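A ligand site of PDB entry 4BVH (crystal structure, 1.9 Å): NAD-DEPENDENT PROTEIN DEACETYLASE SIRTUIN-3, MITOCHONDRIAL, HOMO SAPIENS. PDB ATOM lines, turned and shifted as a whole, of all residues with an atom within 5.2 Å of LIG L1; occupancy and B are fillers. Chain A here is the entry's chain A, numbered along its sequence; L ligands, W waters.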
ATOM      1  N   VAL A  29     -18.485   1.573  23.537  1.00  0.00           N
ATOM      2  CA  VAL A  29     -19.028   0.733  22.468  1.00  0.00           C
ATOM      3  C   VAL A  29     -18.348   1.022  21.112  1.00  0.00           C
ATOM      4  O   VAL A  29     -17.775   2.119  20.842  1.00  0.00           O
ATOM      5  CB  VAL A  29     -20.608   0.852  22.350  1.00  0.00           C
ATOM      6  CG1 VAL A  29     -21.299   0.607  23.719  1.00  0.00           C
ATOM      7  CG2 VAL A  29     -21.055   2.218  21.842  1.00  0.00           C
ATOM      8  N   GLY A  30     -18.436   0.012  20.248  1.00  0.00           N
ATOM      9  CA  GLY A  30     -18.116   0.217  18.824  1.00  0.00           C
ATOM     10  C   GLY A  30     -19.108  -0.510  17.910  1.00  0.00           C
ATOM     11  O   GLY A  30     -20.281  -0.791  18.271  1.00  0.00           O
ATOM     12  N   ALA A  31     -18.628  -0.833  16.705  1.00  0.00           N
ATOM     13  CA  ALA A  31     -19.484  -1.136  15.562  1.00  0.00           C
ATOM     14  C   ALA A  31     -20.199  -2.473  15.725  1.00  0.00           C
ATOM     15  O   ALA A  31     -21.280  -2.747  15.079  1.00  0.00           O
ATOM     16  CB  ALA A  31     -18.618  -1.128  14.313  1.00  0.00           C
ATOM     17  N   GLY A  32     -19.587  -3.331  16.536  1.00  0.00           N
ATOM     18  CA  GLY A  32     -20.177  -4.626  16.864  1.00  0.00           C
ATOM     19  C   GLY A  32     -21.560  -4.475  17.519  1.00  0.00           C
ATOM     20  O   GLY A  32     -22.389  -5.359  17.368  1.00  0.00           O
ATOM     21  N   THR A  35     -24.182  -4.255  14.455  1.00  0.00           N
ATOM     22  CA  THR A  35     -24.400  -5.362  13.518  1.00  0.00           C
ATOM     23  C   THR A  35     -25.754  -6.036  13.689  1.00  0.00           C
ATOM     24  O   THR A  35     -26.341  -6.476  12.694  1.00  0.00           O
ATOM     25  CB  THR A  35     -23.230  -6.349  13.473  1.00  0.00           C
ATOM     26  OG1 THR A  35     -23.078  -7.064  14.722  1.00  0.00           O
ATOM     27  CG2 THR A  35     -21.934  -5.686  13.075  1.00  0.00           C
ATOM     28  N   PRO A  36     -26.241  -6.216  14.939  1.00  0.00           N
ATOM     29  CA  PRO A  36     -27.608  -6.726  15.082  1.00  0.00           C
ATOM     30  C   PRO A  36     -28.698  -5.788  14.566  1.00  0.00           C
ATOM     31  O   PRO A  36     -29.806  -6.244  14.373  1.00  0.00           O
ATOM     32  CB  PRO A  36     -27.761  -6.884  16.626  1.00  0.00           C
ATOM     33  CG  PRO A  36     -26.384  -7.103  17.089  1.00  0.00           C
ATOM     34  CD  PRO A  36     -25.619  -6.054  16.267  1.00  0.00           C
ATOM     35  N   ASP A  41     -19.837  -4.042  10.642  1.00  0.00           N
ATOM     36  CA  ASP A  41     -18.686  -3.460  11.319  1.00  0.00           C
ATOM     37  C   ASP A  41     -17.518  -3.223  10.374  1.00  0.00           C
ATOM     38  O   ASP A  41     -17.689  -3.349   9.182  1.00  0.00           O
ATOM     39  CB  ASP A  41     -18.261  -4.299  12.549  1.00  0.00           C
ATOM     40  CG  ASP A  41     -17.712  -5.687  12.187  1.00  0.00           C
ATOM     41  OD1 ASP A  41     -17.413  -5.963  10.996  1.00  0.00           O
ATOM     42  OD2 ASP A  41     -17.537  -6.525  13.128  1.00  0.00           O
ATOM     43  N   PHE A  42     -16.345  -2.976  10.898  1.00  0.00           N
ATOM     44  CA  PHE A  42     -15.143  -2.839  10.048  1.00  0.00           C
ATOM     45  C   PHE A  42     -14.416  -4.110   9.675  1.00  0.00           C
ATOM     46  O   PHE A  42     -14.126  -4.336   8.484  1.00  0.00           O
ATOM     47  CB  PHE A  42     -14.146  -1.823  10.599  1.00  0.00           C
ATOM     48  CG  PHE A  42     -14.715  -0.449  10.684  1.00  0.00           C
ATOM     49  CD1 PHE A  42     -14.693   0.384   9.590  1.00  0.00           C
ATOM     50  CD2 PHE A  42     -15.375  -0.044  11.820  1.00  0.00           C
ATOM     51  CE1 PHE A  42     -15.232   1.664   9.655  1.00  0.00           C
ATOM     52  CE2 PHE A  42     -15.974   1.212  11.878  1.00  0.00           C
ATOM     53  CZ  PHE A  42     -15.870   2.075  10.802  1.00  0.00           C
ATOM     54  N   ARG A  43     -14.144  -4.926  10.683  1.00  0.00           N
ATOM     55  CA  ARG A  43     -13.051  -5.865  10.666  1.00  0.00           C
ATOM     56  C   ARG A  43     -13.558  -7.321  10.699  1.00  0.00           C
ATOM     57  O   ARG A  43     -12.745  -8.222  10.574  1.00  0.00           O
ATOM     58  CB  ARG A  43     -12.081  -5.533  11.836  1.00  0.00           C
ATOM     59  CG  ARG A  43     -11.331  -4.206  11.653  1.00  0.00           C
ATOM     60  CD  ARG A  43     -10.467  -3.804  12.831  1.00  0.00           C
ATOM     61  NE  ARG A  43      -9.748  -2.531  12.614  1.00  0.00           N
ATOM     62  CZ  ARG A  43     -10.214  -1.290  12.865  1.00  0.00           C
ATOM     63  NH1 ARG A  43     -11.448  -1.064  13.365  1.00  0.00           N
ATOM     64  NH2 ARG A  43      -9.441  -0.240  12.621  1.00  0.00           N
ATOM     65  N   SER A  44     -14.869  -7.566  10.809  1.00  0.00           N
ATOM     66  CA  SER A  44     -15.368  -8.924  10.749  1.00  0.00           C
ATOM     67  C   SER A  44     -15.035  -9.514   9.387  1.00  0.00           C
ATOM     68  O   SER A  44     -15.335  -8.895   8.374  1.00  0.00           O
ATOM     69  CB  SER A  44     -16.864  -9.029  11.018  1.00  0.00           C
ATOM     70  OG  SER A  44     -17.111  -8.891  12.425  1.00  0.00           O
ATOM     71  N   TYR A  50     -14.097  -3.273   5.851  1.00  0.00           N
ATOM     72  CA  TYR A  50     -12.742  -3.188   5.349  1.00  0.00           C
ATOM     73  C   TYR A  50     -12.434  -4.406   4.461  1.00  0.00           C
ATOM     74  O   TYR A  50     -11.406  -4.421   3.774  1.00  0.00           O
ATOM     75  CB  TYR A  50     -11.714  -2.994   6.474  1.00  0.00           C
ATOM     76  CG  TYR A  50     -11.700  -1.591   7.061  1.00  0.00           C
ATOM     77  CD1 TYR A  50     -12.262  -0.516   6.357  1.00  0.00           C
ATOM     78  CD2 TYR A  50     -11.089  -1.322   8.303  1.00  0.00           C
ATOM     79  CE1 TYR A  50     -12.263   0.781   6.870  1.00  0.00           C
ATOM     80  CE2 TYR A  50     -11.085  -0.018   8.839  1.00  0.00           C
ATOM     81  CZ  TYR A  50     -11.665   1.030   8.130  1.00  0.00           C
ATOM     82  OH  TYR A  50     -11.682   2.328   8.656  1.00  0.00           O
ATOM     83  N   PHE A  65     -12.784   6.874   4.978  1.00  0.00           N
ATOM     84  CA  PHE A  65     -13.015   7.578   6.235  1.00  0.00           C
ATOM     85  C   PHE A  65     -11.840   8.470   6.634  1.00  0.00           C
ATOM     86  O   PHE A  65     -11.695   8.775   7.811  1.00  0.00           O
ATOM     87  CB  PHE A  65     -13.377   6.590   7.353  1.00  0.00           C
ATOM     88  CG  PHE A  65     -14.614   5.759   7.063  1.00  0.00           C
ATOM     89  CD1 PHE A  65     -15.833   6.379   6.747  1.00  0.00           C
ATOM     90  CD2 PHE A  65     -14.565   4.367   7.120  1.00  0.00           C
ATOM     91  CE1 PHE A  65     -16.988   5.629   6.504  1.00  0.00           C
ATOM     92  CE2 PHE A  65     -15.705   3.616   6.864  1.00  0.00           C
ATOM     93  CZ  PHE A  65     -16.916   4.243   6.588  1.00  0.00           C
ATOM     94  N   GLN A 113     -17.858   4.935  19.594  1.00  0.00           N
ATOM     95  CA  GLN A 113     -17.081   5.125  18.364  1.00  0.00           C
ATOM     96  C   GLN A 113     -17.951   5.184  17.112  1.00  0.00           C
ATOM     97  O   GLN A 113     -17.467   5.520  16.019  1.00  0.00           O
ATOM     98  CB  GLN A 113     -16.097   3.951  18.186  1.00  0.00           C
ATOM     99  CG  GLN A 113     -15.029   3.951  19.296  1.00  0.00           C
ATOM    100  CD  GLN A 113     -14.253   2.642  19.347  1.00  0.00           C
ATOM    101  OE1 GLN A 113     -13.142   2.565  18.844  1.00  0.00           O
ATOM    102  NE2 GLN A 113     -14.850   1.603  19.931  1.00  0.00           N
ATOM    103  N   ASN A 114     -19.217   4.788  17.242  1.00  0.00           N
ATOM    104  CA  ASN A 114     -20.129   4.707  16.092  1.00  0.00           C
ATOM    105  C   ASN A 114     -20.634   6.070  15.640  1.00  0.00           C
ATOM    106  O   ASN A 114     -20.793   6.995  16.464  1.00  0.00           O
ATOM    107  CB  ASN A 114     -21.334   3.812  16.477  1.00  0.00           C
ATOM    108  CG  ASN A 114     -20.911   2.391  16.802  1.00  0.00           C
ATOM    109  OD1 ASN A 114     -19.790   2.016  16.460  1.00  0.00           O
ATOM    110  ND2 ASN A 114     -21.786   1.582  17.424  1.00  0.00           N
ATOM    111  N   HIS A 133     -16.680   9.923  17.583  1.00  0.00           N
ATOM    112  CA  HIS A 133     -16.426  10.146  16.124  1.00  0.00           C
ATOM    113  C   HIS A 133     -17.432  11.050  15.446  1.00  0.00           C
ATOM    114  O   HIS A 133     -17.623  11.024  14.238  1.00  0.00           O
ATOM    115  CB  HIS A 133     -16.278   8.796  15.416  1.00  0.00           C
ATOM    116  CG  HIS A 133     -15.048   8.069  15.817  1.00  0.00           C
ATOM    117  ND1 HIS A 133     -14.984   6.698  16.000  1.00  0.00           N
ATOM    118  CD2 HIS A 133     -13.808   8.545  16.106  1.00  0.00           C
ATOM    119  CE1 HIS A 133     -13.765   6.354  16.375  1.00  0.00           C
ATOM    120  NE2 HIS A 133     -13.044   7.464  16.488  1.00  0.00           N
ATOM    121  N   VAL A 177     -15.832  12.568  12.592  1.00  0.00           N
ATOM    122  CA  VAL A 177     -14.402  12.579  12.738  1.00  0.00           C
ATOM    123  C   VAL A 177     -13.815  11.556  11.814  1.00  0.00           C
ATOM    124  O   VAL A 177     -13.898  10.343  12.042  1.00  0.00           O
ATOM    125  CB  VAL A 177     -13.944  12.277  14.186  1.00  0.00           C
ATOM    126  CG1 VAL A 177     -12.462  12.518  14.347  1.00  0.00           C
ATOM    127  CG2 VAL A 177     -14.671  13.216  15.121  1.00  0.00           C
ATOM    128  N   PHE A 178     -13.225  12.063  10.742  1.00  0.00           N
ATOM    129  CA  PHE A 178     -12.434  11.254   9.827  1.00  0.00           C
ATOM    130  C   PHE A 178     -11.093  10.896  10.477  1.00  0.00           C
ATOM    131  O   PHE A 178     -10.696  11.525  11.463  1.00  0.00           O
ATOM    132  CB  PHE A 178     -12.271  12.007   8.486  1.00  0.00           C
ATOM    133  CG  PHE A 178     -13.465  11.873   7.564  1.00  0.00           C
ATOM    134  CD1 PHE A 178     -14.510  11.011   7.856  1.00  0.00           C
ATOM    135  CD2 PHE A 178     -13.494  12.539   6.358  1.00  0.00           C
ATOM    136  CE1 PHE A 178     -15.585  10.870   7.001  1.00  0.00           C
ATOM    137  CE2 PHE A 178     -14.561  12.398   5.496  1.00  0.00           C
ATOM    138  CZ  PHE A 178     -15.619  11.564   5.819  1.00  0.00           C
ATOM    139  N   PHE A 179     -10.425   9.876   9.934  1.00  0.00           N
ATOM    140  CA  PHE A 179      -9.075   9.453  10.363  1.00  0.00           C
ATOM    141  C   PHE A 179      -8.108  10.605  10.441  1.00  0.00           C
ATOM    142  O   PHE A 179      -8.053  11.478   9.542  1.00  0.00           O
ATOM    143  CB  PHE A 179      -8.469   8.422   9.414  1.00  0.00           C
ATOM    144  CG  PHE A 179      -8.744   6.994   9.789  1.00  0.00           C
ATOM    145  CD1 PHE A 179      -8.448   6.518  11.069  1.00  0.00           C
ATOM    146  CD2 PHE A 179      -9.273   6.097   8.852  1.00  0.00           C
ATOM    147  CE1 PHE A 179      -8.698   5.195  11.419  1.00  0.00           C
ATOM    148  CE2 PHE A 179      -9.523   4.774   9.202  1.00  0.00           C
ATOM    149  CZ  PHE A 179      -9.230   4.319  10.476  1.00  0.00           C
ATOM    150  N   GLY A 204     -18.772  -4.760  21.816  1.00  0.00           N
ATOM    151  CA  GLY A 204     -18.785  -4.748  20.365  1.00  0.00           C
ATOM    152  C   GLY A 204     -17.703  -3.838  19.797  1.00  0.00           C
ATOM    153  O   GLY A 204     -17.978  -3.015  18.910  1.00  0.00           O
ATOM    154  N   THR A 205     -16.475  -3.928  20.305  1.00  0.00           N
ATOM    155  CA  THR A 205     -15.409  -3.116  19.710  1.00  0.00           C
ATOM    156  C   THR A 205     -14.166  -4.008  19.682  1.00  0.00           C
ATOM    157  O   THR A 205     -13.998  -4.874  20.554  1.00  0.00           O
ATOM    158  CB  THR A 205     -15.172  -1.748  20.397  1.00  0.00           C
ATOM    159  OG1 THR A 205     -13.923  -1.153  19.979  1.00  0.00           O
ATOM    160  CG2 THR A 205     -15.179  -1.837  21.925  1.00  0.00           C
ATOM    161  N   SER A 206     -13.349  -3.841  18.646  1.00  0.00           N
ATOM    162  CA  SER A 206     -12.065  -4.601  18.563  1.00  0.00           C
ATOM    163  C   SER A 206     -10.964  -3.931  19.378  1.00  0.00           C
ATOM    164  O   SER A 206      -9.900  -4.528  19.584  1.00  0.00           O
ATOM    165  CB  SER A 206     -11.603  -4.767  17.089  1.00  0.00           C
ATOM    166  OG  SER A 206     -11.407  -3.476  16.534  1.00  0.00           O
ATOM    167  N   LEU A 207     -11.180  -2.705  19.825  1.00  0.00           N
ATOM    168  CA  LEU A 207     -10.172  -1.980  20.617  1.00  0.00           C
ATOM    169  C   LEU A 207      -8.794  -1.861  19.887  1.00  0.00           C
ATOM    170  O   LEU A 207      -7.731  -1.918  20.523  1.00  0.00           O
ATOM    171  CB  LEU A 207      -9.958  -2.628  21.983  1.00  0.00           C
ATOM    172  CG  LEU A 207     -11.110  -2.512  22.969  1.00  0.00           C
ATOM    173  CD1 LEU A 207     -10.668  -3.203  24.238  1.00  0.00           C
ATOM    174  CD2 LEU A 207     -11.495  -1.050  23.255  1.00  0.00           C
ATOM    175  N   VAL A 209      -8.216   0.721  17.711  1.00  0.00           N
ATOM    176  CA  VAL A 209      -7.923   2.112  17.439  1.00  0.00           C
ATOM    177  C   VAL A 209      -7.764   2.848  18.743  1.00  0.00           C
ATOM    178  O   VAL A 209      -8.555   2.679  19.685  1.00  0.00           O
ATOM    179  CB  VAL A 209      -9.033   2.739  16.577  1.00  0.00           C
ATOM    180  CG1 VAL A 209      -8.814   4.227  16.397  1.00  0.00           C
ATOM    181  CG2 VAL A 209      -9.113   2.026  15.226  1.00  0.00           C
ATOM    182  N   ASN A 229     -18.432  -9.426  23.615  1.00  0.00           N
ATOM    183  CA  ASN A 229     -17.864  -9.229  22.272  1.00  0.00           C
ATOM    184  C   ASN A 229     -17.596 -10.621  21.729  1.00  0.00           C
ATOM    185  O   ASN A 229     -17.496 -11.568  22.506  1.00  0.00           O
ATOM    186  CB  ASN A 229     -16.497  -8.492  22.396  1.00  0.00           C
ATOM    187  CG  ASN A 229     -16.033  -7.900  21.039  1.00  0.00           C
ATOM    188  OD1 ASN A 229     -16.841  -7.277  20.387  1.00  0.00           O
ATOM    189  ND2 ASN A 229     -14.759  -8.114  20.635  1.00  0.00           N
ATOM    190  N   ARG A 230     -17.497 -10.750  20.425  1.00  0.00           N
ATOM    191  CA  ARG A 230     -17.168 -12.019  19.819  1.00  0.00           C
ATOM    192  C   ARG A 230     -15.832 -12.597  20.306  1.00  0.00           C
ATOM    193  O   ARG A 230     -15.792 -13.753  20.665  1.00  0.00           O
ATOM    194  CB  ARG A 230     -17.158 -11.852  18.319  1.00  0.00           C
ATOM    195  CG  ARG A 230     -17.001 -13.125  17.506  1.00  0.00           C
ATOM    196  CD  ARG A 230     -17.259 -12.750  16.044  1.00  0.00           C
ATOM    197  NE  ARG A 230     -18.691 -12.456  15.777  1.00  0.00           N
ATOM    198  CZ  ARG A 230     -19.134 -11.623  14.827  1.00  0.00           C
ATOM    199  NH1 ARG A 230     -18.275 -10.962  14.055  1.00  0.00           N
ATOM    200  NH2 ARG A 230     -20.440 -11.443  14.643  1.00  0.00           N
ATOM    201  N   ASP A 231     -14.790 -11.768  20.390  1.00  0.00           N
ATOM    202  CA  ASP A 231     -13.446 -12.170  20.779  1.00  0.00           C
ATOM    203  C   ASP A 231     -12.925 -11.371  21.919  1.00  0.00           C
ATOM    204  O   ASP A 231     -13.380 -10.223  22.128  1.00  0.00           O
ATOM    205  CB  ASP A 231     -12.498 -11.898  19.641  1.00  0.00           C
ATOM    206  CG  ASP A 231     -12.943 -12.581  18.380  1.00  0.00           C
ATOM    207  OD1 ASP A 231     -13.230 -13.789  18.455  1.00  0.00           O
ATOM    208  OD2 ASP A 231     -13.136 -11.876  17.365  1.00  0.00           O
ATOM    209  N   VAL A 233     -10.178  -9.016  23.296  1.00  0.00           N
ATOM    210  CA  VAL A 233      -9.445  -8.079  22.476  1.00  0.00           C
ATOM    211  C   VAL A 233      -8.724  -7.073  23.307  1.00  0.00           C
ATOM    212  O   VAL A 233      -9.097  -6.828  24.475  1.00  0.00           O
ATOM    213  CB  VAL A 233     -10.364  -7.315  21.473  1.00  0.00           C
ATOM    214  CG1 VAL A 233     -10.877  -8.206  20.350  1.00  0.00           C
ATOM    215  CG2 VAL A 233     -11.532  -6.646  22.207  1.00  0.00           C
ATOM    216  N   GLY A 249     -19.032 -14.158  22.604  1.00  0.00           N
ATOM    217  CA  GLY A 249     -20.155 -14.678  21.861  1.00  0.00           C
ATOM    218  C   GLY A 249     -20.917 -13.520  21.270  1.00  0.00           C
ATOM    219  O   GLY A 249     -20.423 -12.395  21.296  1.00  0.00           O
ATOM    220  N   ASP A 250     -22.149 -13.784  20.785  1.00  0.00           N
ATOM    221  CA  ASP A 250     -22.914 -12.746  20.090  1.00  0.00           C
ATOM    222  C   ASP A 250     -23.240 -11.676  21.141  1.00  0.00           C
ATOM    223  O   ASP A 250     -23.553 -12.015  22.268  1.00  0.00           O
ATOM    224  CB  ASP A 250     -24.202 -13.298  19.480  1.00  0.00           C
ATOM    225  CG  ASP A 250     -25.086 -12.210  18.904  1.00  0.00           C
ATOM    226  OD1 ASP A 250     -24.782 -11.671  17.813  1.00  0.00           O
ATOM    227  OD2 ASP A 250     -26.123 -11.883  19.541  1.00  0.00           O
ATOM    228  N   VAL A 251     -23.267 -10.407  20.741  1.00  0.00           N
ATOM    229  CA  VAL A 251     -23.465  -9.379  21.730  1.00  0.00           C
ATOM    230  C   VAL A 251     -24.923  -9.366  22.257  1.00  0.00           C
ATOM    231  O   VAL A 251     -25.160  -9.059  23.427  1.00  0.00           O
ATOM    232  CB  VAL A 251     -22.993  -7.971  21.202  1.00  0.00           C
ATOM    233  CG1 VAL A 251     -23.868  -7.459  20.050  1.00  0.00           C
ATOM    234  CG2 VAL A 251     -22.982  -6.950  22.304  1.00  0.00           C
ATOM    235  N   VAL A 252     -25.904  -9.661  21.418  1.00  0.00           N
ATOM    236  CA  VAL A 252     -27.270  -9.632  21.898  1.00  0.00           C
ATOM    237  C   VAL A 252     -27.466 -10.787  22.962  1.00  0.00           C
ATOM    238  O   VAL A 252     -28.104 -10.583  24.016  1.00  0.00           O
ATOM    239  CB  VAL A 252     -28.291  -9.748  20.744  1.00  0.00           C
ATOM    240  CG1 VAL A 252     -29.666 -10.037  21.316  1.00  0.00           C
ATOM    241  CG2 VAL A 252     -28.404  -8.439  19.985  1.00  0.00           C
HETATM  242  P1  LIG L   1     -14.442  -3.101  14.547  1.00  0.00           P
HETATM  243  O1  LIG L   1     -12.915  -2.806  14.490  1.00  0.00           O
HETATM  244  O2  LIG L   1     -15.180  -3.511  13.302  1.00  0.00           O
HETATM  245  O3  LIG L   1     -14.716  -4.052  15.832  1.00  0.00           O
HETATM  246  C1  LIG L   1     -16.048  -4.685  15.931  1.00  0.00           C
HETATM  247  C2  LIG L   1     -15.967  -5.715  17.104  1.00  0.00           C
HETATM  248  O4  LIG L   1     -17.276  -6.250  17.318  1.00  0.00           O
HETATM  249  C3  LIG L   1     -15.114  -6.860  16.606  1.00  0.00           C
HETATM  250  O5  LIG L   1     -14.294  -7.298  17.605  1.00  0.00           O
HETATM  251  C4  LIG L   1     -16.154  -7.887  16.145  1.00  0.00           C
HETATM  252  O6  LIG L   1     -15.658  -9.264  16.366  1.00  0.00           O
HETATM  253  C5  LIG L   1     -17.289  -7.652  17.205  1.00  0.00           C
HETATM  254  N1  LIG L   1     -18.624  -7.960  16.756  1.00  0.00           N
HETATM  255  C6  LIG L   1     -19.265  -7.582  15.616  1.00  0.00           C
HETATM  256  N2  LIG L   1     -20.454  -8.082  15.660  1.00  0.00           N
HETATM  257  C7  LIG L   1     -20.661  -8.726  16.813  1.00  0.00           C
HETATM  258  C8  LIG L   1     -21.721  -9.368  17.339  1.00  0.00           C
HETATM  259  N3  LIG L   1     -22.873  -9.440  16.669  1.00  0.00           N
HETATM  260  N4  LIG L   1     -21.660  -9.950  18.578  1.00  0.00           N
HETATM  261  C9  LIG L   1     -20.482  -9.895  19.281  1.00  0.00           C
HETATM  262  N5  LIG L   1     -19.421  -9.210  18.737  1.00  0.00           N
HETATM  263  C10 LIG L   1     -19.538  -8.624  17.509  1.00  0.00           C
HETATM  264  O7  LIG L   1     -15.217  -1.720  15.011  1.00  0.00           O
HETATM  265  P2  LIG L   1     -14.819  -0.694  16.126  1.00  0.00           P
HETATM  266  O8  LIG L   1     -13.986  -1.254  17.245  1.00  0.00           O
HETATM  267  O9  LIG L   1     -15.965   0.199  16.413  1.00  0.00           O
HETATM  268  O10 LIG L   1     -13.149   4.801  13.097  1.00  0.00           O
HETATM  269  O11 LIG L   1     -13.729   0.136  15.228  1.00  0.00           O
HETATM  270  C11 LIG L   1     -13.286   1.350  15.830  1.00  0.00           C
HETATM  271  C12 LIG L   1     -13.005   2.365  14.753  1.00  0.00           C
HETATM  272  O12 LIG L   1     -12.270   1.694  13.698  1.00  0.00           O
HETATM  273  C13 LIG L   1     -14.277   2.860  14.035  1.00  0.00           C
HETATM  274  O13 LIG L   1     -15.109   3.799  14.827  1.00  0.00           O
HETATM  275  C14 LIG L   1     -13.632   3.498  12.752  1.00  0.00           C
HETATM  276  C15 LIG L   1     -12.514   2.436  12.461  1.00  0.00           C
HETATM  277  O14 LIG L   1     -11.229   3.029  12.197  1.00  0.00           O
HETATM  278  C16 LIG L   1     -12.471   5.657  12.264  1.00  0.00           C
HETATM  279  O15 LIG L   1     -11.721   6.546  12.698  1.00  0.00           O
HETATM  280  C17 LIG L   1     -12.739   5.522  10.766  1.00  0.00           C
HETATM  281  N1  LG2 L   2     -21.898   1.553  13.253  1.00  0.00           N
HETATM  282  O1  LG2 L   2     -21.299   3.691  13.186  1.00  0.00           O
HETATM  283  C1  LG2 L   2     -21.046   2.534  12.858  1.00  0.00           C
HETATM  284  N2  LG2 L   2     -18.115   3.996  12.999  1.00  0.00           N
HETATM  285  C2  LG2 L   2     -19.237   3.528   9.606  1.00  0.00           C
HETATM  286  C3  LG2 L   2     -16.527   5.924  12.891  1.00  0.00           C
HETATM  287  C4  LG2 L   2     -15.938   6.885  12.098  1.00  0.00           C
HETATM  288  C5  LG2 L   2     -17.432   5.001  12.397  1.00  0.00           C
HETATM  289 CL1  LG2 L   2     -15.604   8.113   9.571  1.00  0.00          CL
HETATM  290  C6  LG2 L   2     -17.733   4.961  11.088  1.00  0.00           C
HETATM  291  C7  LG2 L   2     -17.188   5.896  10.275  1.00  0.00           C
HETATM  292  C8  LG2 L   2     -18.625   3.939  10.854  1.00  0.00           C
HETATM  293  C9  LG2 L   2     -18.865   3.304  12.062  1.00  0.00           C
HETATM  294  C10 LG2 L   2     -16.290   6.861  10.758  1.00  0.00           C
HETATM  295  C11 LG2 L   2     -20.463   2.506   9.801  1.00  0.00           C
HETATM  296  C12 LG2 L   2     -19.774   2.149  12.228  1.00  0.00           C
HETATM  297  C13 LG2 L   2     -20.010   1.396  10.848  1.00  0.00           C
HETATM  298  O   HOH W   1     -12.518  -9.330  16.865  1.00  0.00           O
HETATM  299  O   HOH W   2     -13.116  -9.383  14.169  1.00  0.00           O
HETATM  300  O   HOH W   3     -17.445   2.329  15.315  1.00  0.00           O
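An oxygen (O2) of LIG L1 sits at hydrogen-bond distance from the backbone NH (N) of Arg 43 (3.2 Å).
The guanidinium group of Arg 43 is in salt-bridge range of an oxygen (O1) of LIG L1, at 2.5 Å.
The backbone NH (N) of Ser 206 lies within hydrogen-bond range of an oxygen (O8) of LIG L1 (3.0 Å).
OG of Ser 206 is in hydrogen-bond range of O1 of LIG L1 (2.6 Å).
N of Phe 42 lies within hydrogen-bond range of O2 of LIG L1.
A nitrogen (N4) of LIG L1 is in hydrogen-bond range of the backbone NH (N) of Val 251 (2.7 Å).
OG1 of Thr 205 sits at hydrogen-bond distance from O8 of LIG L1 (2.7 Å).
The backbone NH (N) of Ala 31 sits at hydrogen-bond distance from an oxygen (O9) of LIG L1, at 2.9 Å.
The side-chain hydroxyl (OG1) of Thr 35 lies within hydrogen-bond range of a nitrogen (N2) of LIG L1 (3.0 Å).
The backbone NH (N) of Arg 230 is in hydrogen-bond range of a nitrogen (N5) of LIG L1, 3.0 Å away.
A ring nitrogen (ND1) of His 133 sits at hydrogen-bond distance from an oxygen (O13) of LIG L1, 3.1 Å away.
OD1 of Asp 250 lies within hydrogen-bond range of N3 of LIG L1 (3.2 Å).
An oxygen (O13) of LIG L1 sits at hydrogen-bond distance from the backbone carbonyl oxygen of Gln 113 (3.2 Å).
The side-chain amide nitrogen (ND2) of Asn 229 is in hydrogen-bond range of an oxygen (O5) of LIG L1.
A nitrogen (N2) of LG2 L2 lies close to the backbone carbonyl oxygen (O) of Gln 113 (3.4 Å).
The backbone carbonyl oxygen of Phe 42 is in hydrogen-bond range of the backbone NH of Tyr 50 (2.8 Å).
The side-chain hydroxyl of Thr 205 lies within hydrogen-bond range of the backbone NH of Leu 207 (3.2 Å).
The backbone NH (N) of Ala 31 sits at hydrogen-bond distance from the side-chain amide oxygen (OD1) of Asn 114 (3.1 Å).
The backbone carbonyl oxygen of Gly 32 is in hydrogen-bond range of the side-chain hydroxyl of Thr 35, 3.2 Å away.
The guanidinium group (NH1) of Arg 230 sits at hydrogen-bond distance from the side-chain hydroxyl (OG) of Ser 44, 2.9 Å away.
N of Gln 113 sits at hydrogen-bond distance from O of Val 29, 3.1 Å away.
The backbone NH (N) of Gly 204 lies close to the side-chain amide oxygen (OD1) of Asn 229.
The backbone carbonyl oxygen of Gly 30 sits at hydrogen-bond distance from the side-chain amide nitrogen of Asn 114 (2.9 Å).
Gly 30 touches LIG L1.
CA of Gly 32 touches C6 of LIG L1 (3.3 Å).
Asp 41 touches LIG L1.
OG of Ser 44 touches C4 of LIG L1 (3.97 Å).
OH of Tyr 50 touches O14 of LIG L1, 3.6 Å away.
CB of Phe 65 touches C17 of LIG L1, at 3.6 Å.
Phe 179 touches LIG L1.
Gly 204 touches LIG L1.
Val 209 touches LIG L1.
Asp 231 touches LIG L1.
Gly 249 touches LIG L1.
Hydrophobic or aromatic side chains that line LIG L1: Ala 31, Phe 42, Phe 65, His 133, Phe 179, Val 209 and Val 251.
Of the 31 residues printed, 23 come within 4 Å of LIG L1.
Along chain A the residues within 4 Å of LIG L1 span positions 30 to 251.
The nearest printed residue that does not touch LIG L1 is Leu 207 (4.1 Å).
Water W1 lies within hydrogen-bond range of OD2 of Asp 231 (2.7 Å) and O5 of LIG L1 (2.8 Å).
Water W3 lies within hydrogen-bond range of OD1 of Asn 114 (2.6 Å), O13 of LIG L1 (2.8 Å), N2 of LG2 L2 (2.9 Å) and O of Gln 113 (3.3 Å).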
